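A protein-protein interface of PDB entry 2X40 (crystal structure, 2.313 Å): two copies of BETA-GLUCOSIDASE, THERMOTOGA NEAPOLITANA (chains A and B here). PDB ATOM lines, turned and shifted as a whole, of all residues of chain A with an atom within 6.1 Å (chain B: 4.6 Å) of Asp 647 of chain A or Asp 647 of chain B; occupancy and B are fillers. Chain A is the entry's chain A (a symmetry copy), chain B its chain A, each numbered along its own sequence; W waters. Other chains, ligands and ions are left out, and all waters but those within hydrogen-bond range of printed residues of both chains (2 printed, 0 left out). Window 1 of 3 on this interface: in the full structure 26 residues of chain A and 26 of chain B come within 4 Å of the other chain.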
ATOM      1  N   SER A 182      23.107  14.091   6.577  1.00  0.00           N
ATOM      2  CA  SER A 182      22.573  15.441   6.627  1.00  0.00           C
ATOM      3  C   SER A 182      23.364  16.231   7.653  1.00  0.00           C
ATOM      4  O   SER A 182      23.899  15.668   8.607  1.00  0.00           O
ATOM      5  CB  SER A 182      21.088  15.441   6.995  1.00  0.00           C
ATOM      6  OG  SER A 182      20.902  15.271   8.388  1.00  0.00           O
ATOM      7  N   ARG A 184      22.112  18.080   9.831  1.00  0.00           N
ATOM      8  CA  ARG A 184      21.383  17.937  11.094  1.00  0.00           C
ATOM      9  C   ARG A 184      21.806  16.706  11.890  1.00  0.00           C
ATOM     10  O   ARG A 184      22.033  16.794  13.099  1.00  0.00           O
ATOM     11  CB  ARG A 184      19.866  17.908  10.896  1.00  0.00           C
ATOM     12  CG  ARG A 184      19.129  17.600  12.195  1.00  0.00           C
ATOM     13  CD  ARG A 184      17.621  17.756  12.106  1.00  0.00           C
ATOM     14  NE  ARG A 184      17.028  17.809  13.443  1.00  0.00           N
ATOM     15  CZ  ARG A 184      15.721  17.760  13.697  1.00  0.00           C
ATOM     16  NH1 ARG A 184      14.847  17.645  12.705  1.00  0.00           N
ATOM     17  NH2 ARG A 184      15.288  17.818  14.949  1.00  0.00           N
ATOM     18  N   ALA A 185      21.898  15.557  11.225  1.00  0.00           N
ATOM     19  CA  ALA A 185      22.330  14.336  11.911  1.00  0.00           C
ATOM     20  C   ALA A 185      23.769  14.490  12.392  1.00  0.00           C
ATOM     21  O   ALA A 185      24.137  14.023  13.472  1.00  0.00           O
ATOM     22  CB  ALA A 185      22.199  13.120  11.000  1.00  0.00           C
ATOM     23  N   GLU A 574      18.160   7.040   8.157  1.00  0.00           N
ATOM     24  CA  GLU A 574      17.457   7.179   9.431  1.00  0.00           C
ATOM     25  C   GLU A 574      17.837   8.484  10.126  1.00  0.00           C
ATOM     26  O   GLU A 574      17.131   8.952  11.020  1.00  0.00           O
ATOM     27  CB  GLU A 574      17.703   5.969  10.346  1.00  0.00           C
ATOM     28  CG  GLU A 574      19.058   5.965  11.058  1.00  0.00           C
ATOM     29  CD  GLU A 574      20.232   5.740  10.117  1.00  0.00           C
ATOM     30  OE1 GLU A 574      21.383   5.952  10.549  1.00  0.00           O
ATOM     31  OE2 GLU A 574      20.012   5.348   8.948  1.00  0.00           O
ATOM     32  N   ASP A 575      18.961   9.061   9.713  1.00  0.00           N
ATOM     33  CA  ASP A 575      19.310  10.408  10.133  1.00  0.00           C
ATOM     34  C   ASP A 575      19.438  10.501  11.655  1.00  0.00           C
ATOM     35  O   ASP A 575      20.110   9.677  12.272  1.00  0.00           O
ATOM     36  CB  ASP A 575      18.246  11.379   9.618  1.00  0.00           C
ATOM     37  CG  ASP A 575      18.764  12.797   9.482  1.00  0.00           C
ATOM     38  OD1 ASP A 575      18.776  13.523  10.500  1.00  0.00           O
ATOM     39  OD2 ASP A 575      19.141  13.188   8.354  1.00  0.00           O
ATOM     40  N   ILE A 576      18.789  11.490  12.267  1.00  0.00           N
ATOM     41  CA  ILE A 576      18.920  11.690  13.710  1.00  0.00           C
ATOM     42  C   ILE A 576      18.239  10.591  14.511  1.00  0.00           C
ATOM     43  O   ILE A 576      18.463  10.469  15.715  1.00  0.00           O
ATOM     44  CB  ILE A 576      18.313  13.024  14.177  1.00  0.00           C
ATOM     45  CG1 ILE A 576      16.840  13.099  13.789  1.00  0.00           C
ATOM     46  CG2 ILE A 576      19.092  14.206  13.625  1.00  0.00           C
ATOM     47  CD1 ILE A 576      16.116  14.255  14.449  1.00  0.00           C
ATOM     48  N   TYR A 577      17.395   9.810  13.849  1.00  0.00           N
ATOM     49  CA  TYR A 577      16.606   8.790  14.524  1.00  0.00           C
ATOM     50  C   TYR A 577      17.387   7.485  14.580  1.00  0.00           C
ATOM     51  O   TYR A 577      17.037   6.495  13.944  1.00  0.00           O
ATOM     52  CB  TYR A 577      15.269   8.614  13.818  1.00  0.00           C
ATOM     53  CG  TYR A 577      14.465   9.877  13.858  1.00  0.00           C
ATOM     54  CD1 TYR A 577      14.345  10.684  12.737  1.00  0.00           C
ATOM     55  CD2 TYR A 577      13.863  10.293  15.036  1.00  0.00           C
ATOM     56  CE1 TYR A 577      13.621  11.855  12.778  1.00  0.00           C
ATOM     57  CE2 TYR A 577      13.147  11.471  15.092  1.00  0.00           C
ATOM     58  CZ  TYR A 577      13.025  12.248  13.959  1.00  0.00           C
ATOM     59  OH  TYR A 577      12.306  13.426  14.012  1.00  0.00           O
ATOM     60  N   LYS A 643       6.604  19.558  20.415  1.00  0.00           N
ATOM     61  CA  LYS A 643       6.657  19.377  18.966  1.00  0.00           C
ATOM     62  C   LYS A 643       6.997  20.684  18.235  1.00  0.00           C
ATOM     63  O   LYS A 643       7.859  20.706  17.356  1.00  0.00           O
ATOM     64  CB  LYS A 643       5.377  18.719  18.430  1.00  0.00           C
ATOM     65  CG  LYS A 643       5.245  17.255  18.835  1.00  0.00           C
ATOM     66  CD  LYS A 643       6.572  16.535  18.611  1.00  0.00           C
ATOM     67  CE  LYS A 643       6.535  15.079  19.040  1.00  0.00           C
ATOM     68  NZ  LYS A 643       7.825  14.393  18.736  1.00  0.00           N
ATOM     69  N   LYS A 645       7.997  23.567  16.106  1.00  0.00           N
ATOM     70  CA  LYS A 645       8.229  23.889  14.700  1.00  0.00           C
ATOM     71  C   LYS A 645       8.704  22.694  13.893  1.00  0.00           C
ATOM     72  O   LYS A 645       8.194  22.418  12.811  1.00  0.00           O
ATOM     73  CB  LYS A 645       9.279  24.995  14.567  1.00  0.00           C
ATOM     74  CG  LYS A 645       9.150  26.137  15.558  1.00  0.00           C
ATOM     75  CD  LYS A 645       8.352  27.282  14.983  1.00  0.00           C
ATOM     76  CE  LYS A 645       8.745  28.598  15.633  1.00  0.00           C
ATOM     77  NZ  LYS A 645      10.152  28.963  15.313  1.00  0.00           N
ATOM     78  N   ILE A 646       9.697  21.995  14.418  1.00  0.00           N
ATOM     79  CA  ILE A 646      10.376  20.969  13.650  1.00  0.00           C
ATOM     80  C   ILE A 646      10.250  19.615  14.328  1.00  0.00           C
ATOM     81  O   ILE A 646      10.039  19.540  15.537  1.00  0.00           O
ATOM     82  CB  ILE A 646      11.860  21.331  13.465  1.00  0.00           C
ATOM     83  CG1 ILE A 646      12.519  20.404  12.444  1.00  0.00           C
ATOM     84  CG2 ILE A 646      12.593  21.313  14.815  1.00  0.00           C
ATOM     85  CD1 ILE A 646      13.910  20.844  12.032  1.00  0.00           C
ATOM     86  N   ASP A 647      10.365  18.548  13.544  1.00  0.00           N
ATOM     87  CA  ASP A 647      10.322  17.192  14.080  1.00  0.00           C
ATOM     88  C   ASP A 647      11.490  16.922  15.037  1.00  0.00           C
ATOM     89  O   ASP A 647      12.619  17.354  14.797  1.00  0.00           O
ATOM     90  CB  ASP A 647      10.318  16.164  12.946  1.00  0.00           C
ATOM     91  CG  ASP A 647      11.517  16.296  12.030  1.00  0.00           C
ATOM     92  OD1 ASP A 647      11.745  17.412  11.513  1.00  0.00           O
ATOM     93  OD2 ASP A 647      12.225  15.282  11.821  1.00  0.00           O
ATOM     94  N   LYS A 648      11.207  16.210  16.122  1.00  0.00           N
ATOM     95  CA  LYS A 648      12.227  15.875  17.111  1.00  0.00           C
ATOM     96  C   LYS A 648      12.015  14.462  17.621  1.00  0.00           C
ATOM     97  O   LYS A 648      10.891  13.956  17.611  1.00  0.00           O
ATOM     98  CB  LYS A 648      12.168  16.839  18.299  1.00  0.00           C
ATOM     99  CG  LYS A 648      12.301  18.312  17.948  1.00  0.00           C
ATOM    100  CD  LYS A 648      12.261  19.156  19.219  1.00  0.00           C
ATOM    101  CE  LYS A 648      12.125  20.644  18.921  1.00  0.00           C
ATOM    102  NZ  LYS A 648      10.789  20.960  18.340  1.00  0.00           N
ATOM    103  N   PRO A 649      13.092  13.816  18.081  1.00  0.00           N
ATOM    104  CA  PRO A 649      12.907  12.497  18.688  1.00  0.00           C
ATOM    105  C   PRO A 649      11.933  12.560  19.861  1.00  0.00           C
ATOM    106  O   PRO A 649      11.685  13.629  20.424  1.00  0.00           O
ATOM    107  CB  PRO A 649      14.313  12.132  19.176  1.00  0.00           C
ATOM    108  CG  PRO A 649      15.228  12.895  18.282  1.00  0.00           C
ATOM    109  CD  PRO A 649      14.513  14.197  17.998  1.00  0.00           C
ATOM    110  N   SER A 681      17.651  21.977  19.089  1.00  0.00           N
ATOM    111  CA  SER A 681      17.668  21.105  17.915  1.00  0.00           C
ATOM    112  C   SER A 681      18.231  21.897  16.750  1.00  0.00           C
ATOM    113  O   SER A 681      18.057  23.113  16.681  1.00  0.00           O
ATOM    114  CB  SER A 681      16.260  20.629  17.551  1.00  0.00           C
ATOM    115  OG  SER A 681      15.778  19.681  18.482  1.00  0.00           O
ATOM    116  N   PHE A 682      18.899  21.212  15.830  1.00  0.00           N
ATOM    117  CA  PHE A 682      19.463  21.874  14.664  1.00  0.00           C
ATOM    118  C   PHE A 682      18.497  21.826  13.476  1.00  0.00           C
ATOM    119  O   PHE A 682      18.056  20.750  13.065  1.00  0.00           O
ATOM    120  CB  PHE A 682      20.790  21.229  14.289  1.00  0.00           C
ATOM    121  CG  PHE A 682      21.602  22.045  13.334  1.00  0.00           C
ATOM    122  CD1 PHE A 682      21.709  21.675  12.005  1.00  0.00           C
ATOM    123  CD2 PHE A 682      22.248  23.199  13.766  1.00  0.00           C
ATOM    124  CE1 PHE A 682      22.454  22.431  11.123  1.00  0.00           C
ATOM    125  CE2 PHE A 682      22.997  23.963  12.892  1.00  0.00           C
ATOM    126  CZ  PHE A 682      23.101  23.582  11.566  1.00  0.00           C
ATOM    127  N   SER B 182       3.867  18.945  14.998  1.00  0.00           N
ATOM    128  CA  SER B 182       4.886  19.938  14.706  1.00  0.00           C
ATOM    129  C   SER B 182       4.428  20.757  13.513  1.00  0.00           C
ATOM    130  O   SER B 182       3.677  20.274  12.668  1.00  0.00           O
ATOM    131  CB  SER B 182       6.235  19.281  14.406  1.00  0.00           C
ATOM    132  OG  SER B 182       6.282  18.783  13.082  1.00  0.00           O
ATOM    133  N   ARG B 184       6.217  21.498  11.068  1.00  0.00           N
ATOM    134  CA  ARG B 184       6.778  20.836   9.888  1.00  0.00           C
ATOM    135  C   ARG B 184       5.874  19.739   9.332  1.00  0.00           C
ATOM    136  O   ARG B 184       5.651  19.670   8.121  1.00  0.00           O
ATOM    137  CB  ARG B 184       8.169  20.252  10.149  1.00  0.00           C
ATOM    138  CG  ARG B 184       8.672  19.431   8.967  1.00  0.00           C
ATOM    139  CD  ARG B 184      10.123  18.996   9.085  1.00  0.00           C
ATOM    140  NE  ARG B 184      10.634  18.548   7.789  1.00  0.00           N
ATOM    141  CZ  ARG B 184      11.804  17.940   7.602  1.00  0.00           C
ATOM    142  NH1 ARG B 184      12.603  17.689   8.633  1.00  0.00           N
ATOM    143  NH2 ARG B 184      12.174  17.576   6.382  1.00  0.00           N
ATOM    144  N   ASP B 575       5.572  12.181  13.082  1.00  0.00           N
ATOM    145  CA  ASP B 575       5.764  13.445  12.393  1.00  0.00           C
ATOM    146  C   ASP B 575       5.620  13.280  10.877  1.00  0.00           C
ATOM    147  O   ASP B 575       4.654  12.684  10.407  1.00  0.00           O
ATOM    148  CB  ASP B 575       7.144  14.001  12.749  1.00  0.00           C
ATOM    149  CG  ASP B 575       7.231  15.505  12.583  1.00  0.00           C
ATOM    150  OD1 ASP B 575       7.463  15.962  11.442  1.00  0.00           O
ATOM    151  OD2 ASP B 575       7.084  16.226  13.596  1.00  0.00           O
ATOM    152  N   TYR B 577       7.137  11.426   8.947  1.00  0.00           N
ATOM    153  CA  TYR B 577       7.434  10.067   8.518  1.00  0.00           C
ATOM    154  C   TYR B 577       6.201   9.191   8.687  1.00  0.00           C
ATOM    155  O   TYR B 577       6.160   8.288   9.520  1.00  0.00           O
ATOM    156  CB  TYR B 577       8.621   9.522   9.298  1.00  0.00           C
ATOM    157  CG  TYR B 577       9.855  10.333   9.044  1.00  0.00           C
ATOM    158  CD1 TYR B 577      10.327  11.231   9.989  1.00  0.00           C
ATOM    159  CD2 TYR B 577      10.524  10.240   7.833  1.00  0.00           C
ATOM    160  CE1 TYR B 577      11.451  11.991   9.748  1.00  0.00           C
ATOM    161  CE2 TYR B 577      11.642  11.005   7.576  1.00  0.00           C
ATOM    162  CZ  TYR B 577      12.105  11.878   8.537  1.00  0.00           C
ATOM    163  OH  TYR B 577      13.226  12.643   8.284  1.00  0.00           O
ATOM    164  N   LYS B 645      21.084  19.649   4.416  1.00  0.00           N
ATOM    165  CA  LYS B 645      21.055  20.305   5.721  1.00  0.00           C
ATOM    166  C   LYS B 645      20.182  19.577   6.727  1.00  0.00           C
ATOM    167  O   LYS B 645      20.586  19.341   7.862  1.00  0.00           O
ATOM    168  CB  LYS B 645      20.530  21.738   5.591  1.00  0.00           C
ATOM    169  CG  LYS B 645      21.057  22.519   4.402  1.00  0.00           C
ATOM    170  CD  LYS B 645      22.264  23.346   4.773  1.00  0.00           C
ATOM    171  CE  LYS B 645      22.393  24.555   3.862  1.00  0.00           C
ATOM    172  NZ  LYS B 645      21.257  25.499   4.045  1.00  0.00           N
ATOM    173  N   ILE B 646      18.973  19.236   6.309  1.00  0.00           N
ATOM    174  CA  ILE B 646      17.978  18.732   7.236  1.00  0.00           C
ATOM    175  C   ILE B 646      17.534  17.333   6.843  1.00  0.00           C
ATOM    176  O   ILE B 646      17.649  16.945   5.682  1.00  0.00           O
ATOM    177  CB  ILE B 646      16.764  19.677   7.286  1.00  0.00           C
ATOM    178  CG1 ILE B 646      15.836  19.304   8.441  1.00  0.00           C
ATOM    179  CG2 ILE B 646      16.029  19.683   5.936  1.00  0.00           C
ATOM    180  CD1 ILE B 646      14.747  20.326   8.702  1.00  0.00           C
ATOM    181  N   ASP B 647      17.041  16.573   7.816  1.00  0.00           N
ATOM    182  CA  ASP B 647      16.525  15.233   7.559  1.00  0.00           C
ATOM    183  C   ASP B 647      15.308  15.261   6.627  1.00  0.00           C
ATOM    184  O   ASP B 647      14.450  16.141   6.731  1.00  0.00           O
ATOM    185  CB  ASP B 647      16.171  14.531   8.871  1.00  0.00           C
ATOM    186  CG  ASP B 647      15.160  15.300   9.695  1.00  0.00           C
ATOM    187  OD1 ASP B 647      15.409  16.494   9.972  1.00  0.00           O
ATOM    188  OD2 ASP B 647      14.119  14.709  10.069  1.00  0.00           O
ATOM    189  N   LYS B 648      15.244  14.298   5.714  1.00  0.00           N
ATOM    190  CA  LYS B 648      14.135  14.204   4.770  1.00  0.00           C
ATOM    191  C   LYS B 648      13.754  12.751   4.557  1.00  0.00           C
ATOM    192  O   LYS B 648      14.588  11.856   4.711  1.00  0.00           O
ATOM    193  CB  LYS B 648      14.520  14.813   3.420  1.00  0.00           C
ATOM    194  CG  LYS B 648      14.991  16.258   3.468  1.00  0.00           C
ATOM    195  CD  LYS B 648      15.308  16.751   2.060  1.00  0.00           C
ATOM    196  CE  LYS B 648      16.029  18.092   2.064  1.00  0.00           C
ATOM    197  NZ  LYS B 648      17.404  17.965   2.626  1.00  0.00           N
HETATM  198  O   HOH W   1      17.733  12.335   6.115  1.00  0.00           O
HETATM  199  O   HOH W   2       8.133  15.347  16.014  1.00  0.00           O
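Among the printed residues, pairs that only touch across the chains: Ser 182 of chain A with Ile 646 of chain B (3.98 Å), Asp 575 of chain A with Asp 647 of chain B (3.2 Å), Tyr 577 of chain A with Tyr 577 of chain B (3.7 Å), Tyr 577 of chain A with Asp 647 of chain B (3.97 Å), Lys 643 of chain A with Ser 182 of chain B (3.7 Å), Ile 646 of chain A with Ser 182 of chain B (3.98 Å), Ile 646 of chain A with Ile 646 of chain B (3.5 Å), Asp 647 of chain A with Asp 575 of chain B (3.2 Å) and Asp 647 of chain A with Tyr 577 of chain B (3.97 Å).
Water W2 lies within hydrogen-bond range of OD2 of Asp 575 of chain B, NZ of Lys 643 of chain A and N of Lys 648 of chain A.
Water W1 lies within hydrogen-bond range of the side-chain carboxylate of Asp 575 of chain A (2.8 Å) and the backbone NH of Lys 648 of chain B (3.2 Å).
The backbone NH (N) of Arg 184 of chain B is in hydrogen-bond range of the backbone carbonyl oxygen (O) of Lys 645 of chain A, at 2.8 Å.
The guanidinium group (NH1) of Arg 184 of chain B lies within salt-bridge range of the side-chain carboxylate (OD1) of Asp 647 of chain A.
O of Lys 645 of chain B sits at hydrogen-bond distance from N of Arg 184 of chain A (2.8 Å).
OD1 of Asp 647 of chain B is in salt-bridge range of NH1 of Arg 184 of chain A, at 3.0 Å.
The side-chain carboxylate (OD2) of Asp 647 of chain A sits close to the side-chain carboxylate (OD2) of Asp 647 of chain B (2.6 Å).
Of the printed residues of chain B, Ser 182 of chain A touches Ile 646 (3.98 Å).
Printed residues of chain B within 4 Å of Ile 646 of chain A: Ser 182 and Ile 646.
Lys 648 of chain A touches none of the printed residues of chain B.
Pro 649 of chain A touches none of the printed residues of chain B.
Of the printed residues of chain A, Arg 184 of chain B touches Lys 645 (2.8 Å) and Asp 647 (3.0 Å).
Printed residues of chain A within 4 Å of Ile 646 of chain B: Ser 182 (3.98 Å) and Ile 646 (3.5 Å).
Asp 647 of chain B touches four residues of chain A.
The nearest residue of chain A that does not touch Asp 647 of chain B is Ser 182 of chain A (4.1 Å).
OD1 of Asp 647 of chain B is in salt-bridge range of NH1 of Arg 184 of chain B (3.3 Å).
OH of Tyr 577 of chain B is in hydrogen-bond range of OD2 of Asp 647 of chain B (2.9 Å).
The backbone NH (N) of Arg 184 of chain A lies close to the side-chain hydroxyl (OG) of Ser 182 of chain A, 3.4 Å away.
The guanidinium group of Arg 184 of chain A sits at hydrogen-bond distance from the backbone carbonyl oxygen of Phe 682 of chain A, at 3.1 Å.
OD2 of Asp 647 of chain A lies within hydrogen-bond range of OH of Tyr 577 of chain A (2.9 Å).
The side-chain amino group of Lys 648 of chain A is in hydrogen-bond range of the backbone carbonyl oxygen of Lys 643 of chain A.
Of the 8 printed residues of chain B, 7 touch a printed residue of chain A.
Among the printed residues, Asp or Glu carboxylates within 4 Å of a Lys or Arg side-chain nitrogen of the other chain: Arg 184 of chain A with Asp 647 of chain B (3.0 Å) and Asp 647 of chain A with Arg 184 of chain B (3.0 Å).
Ser 182 of chain A touches Ile 646 of chain B, and with the chains exchanged Ile 646 of chain A touches Ser 182 of chain B.
Arg 184 of chain A touches Lys 645 of chain B, and with the chains exchanged Lys 645 of chain A touches Arg 184 of chain B.
Ile 646 of chain A touches its own counterpart, Ile 646 of chain B.
Asp 647 of chain A touches its own counterpart, Asp 647 of chain B.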
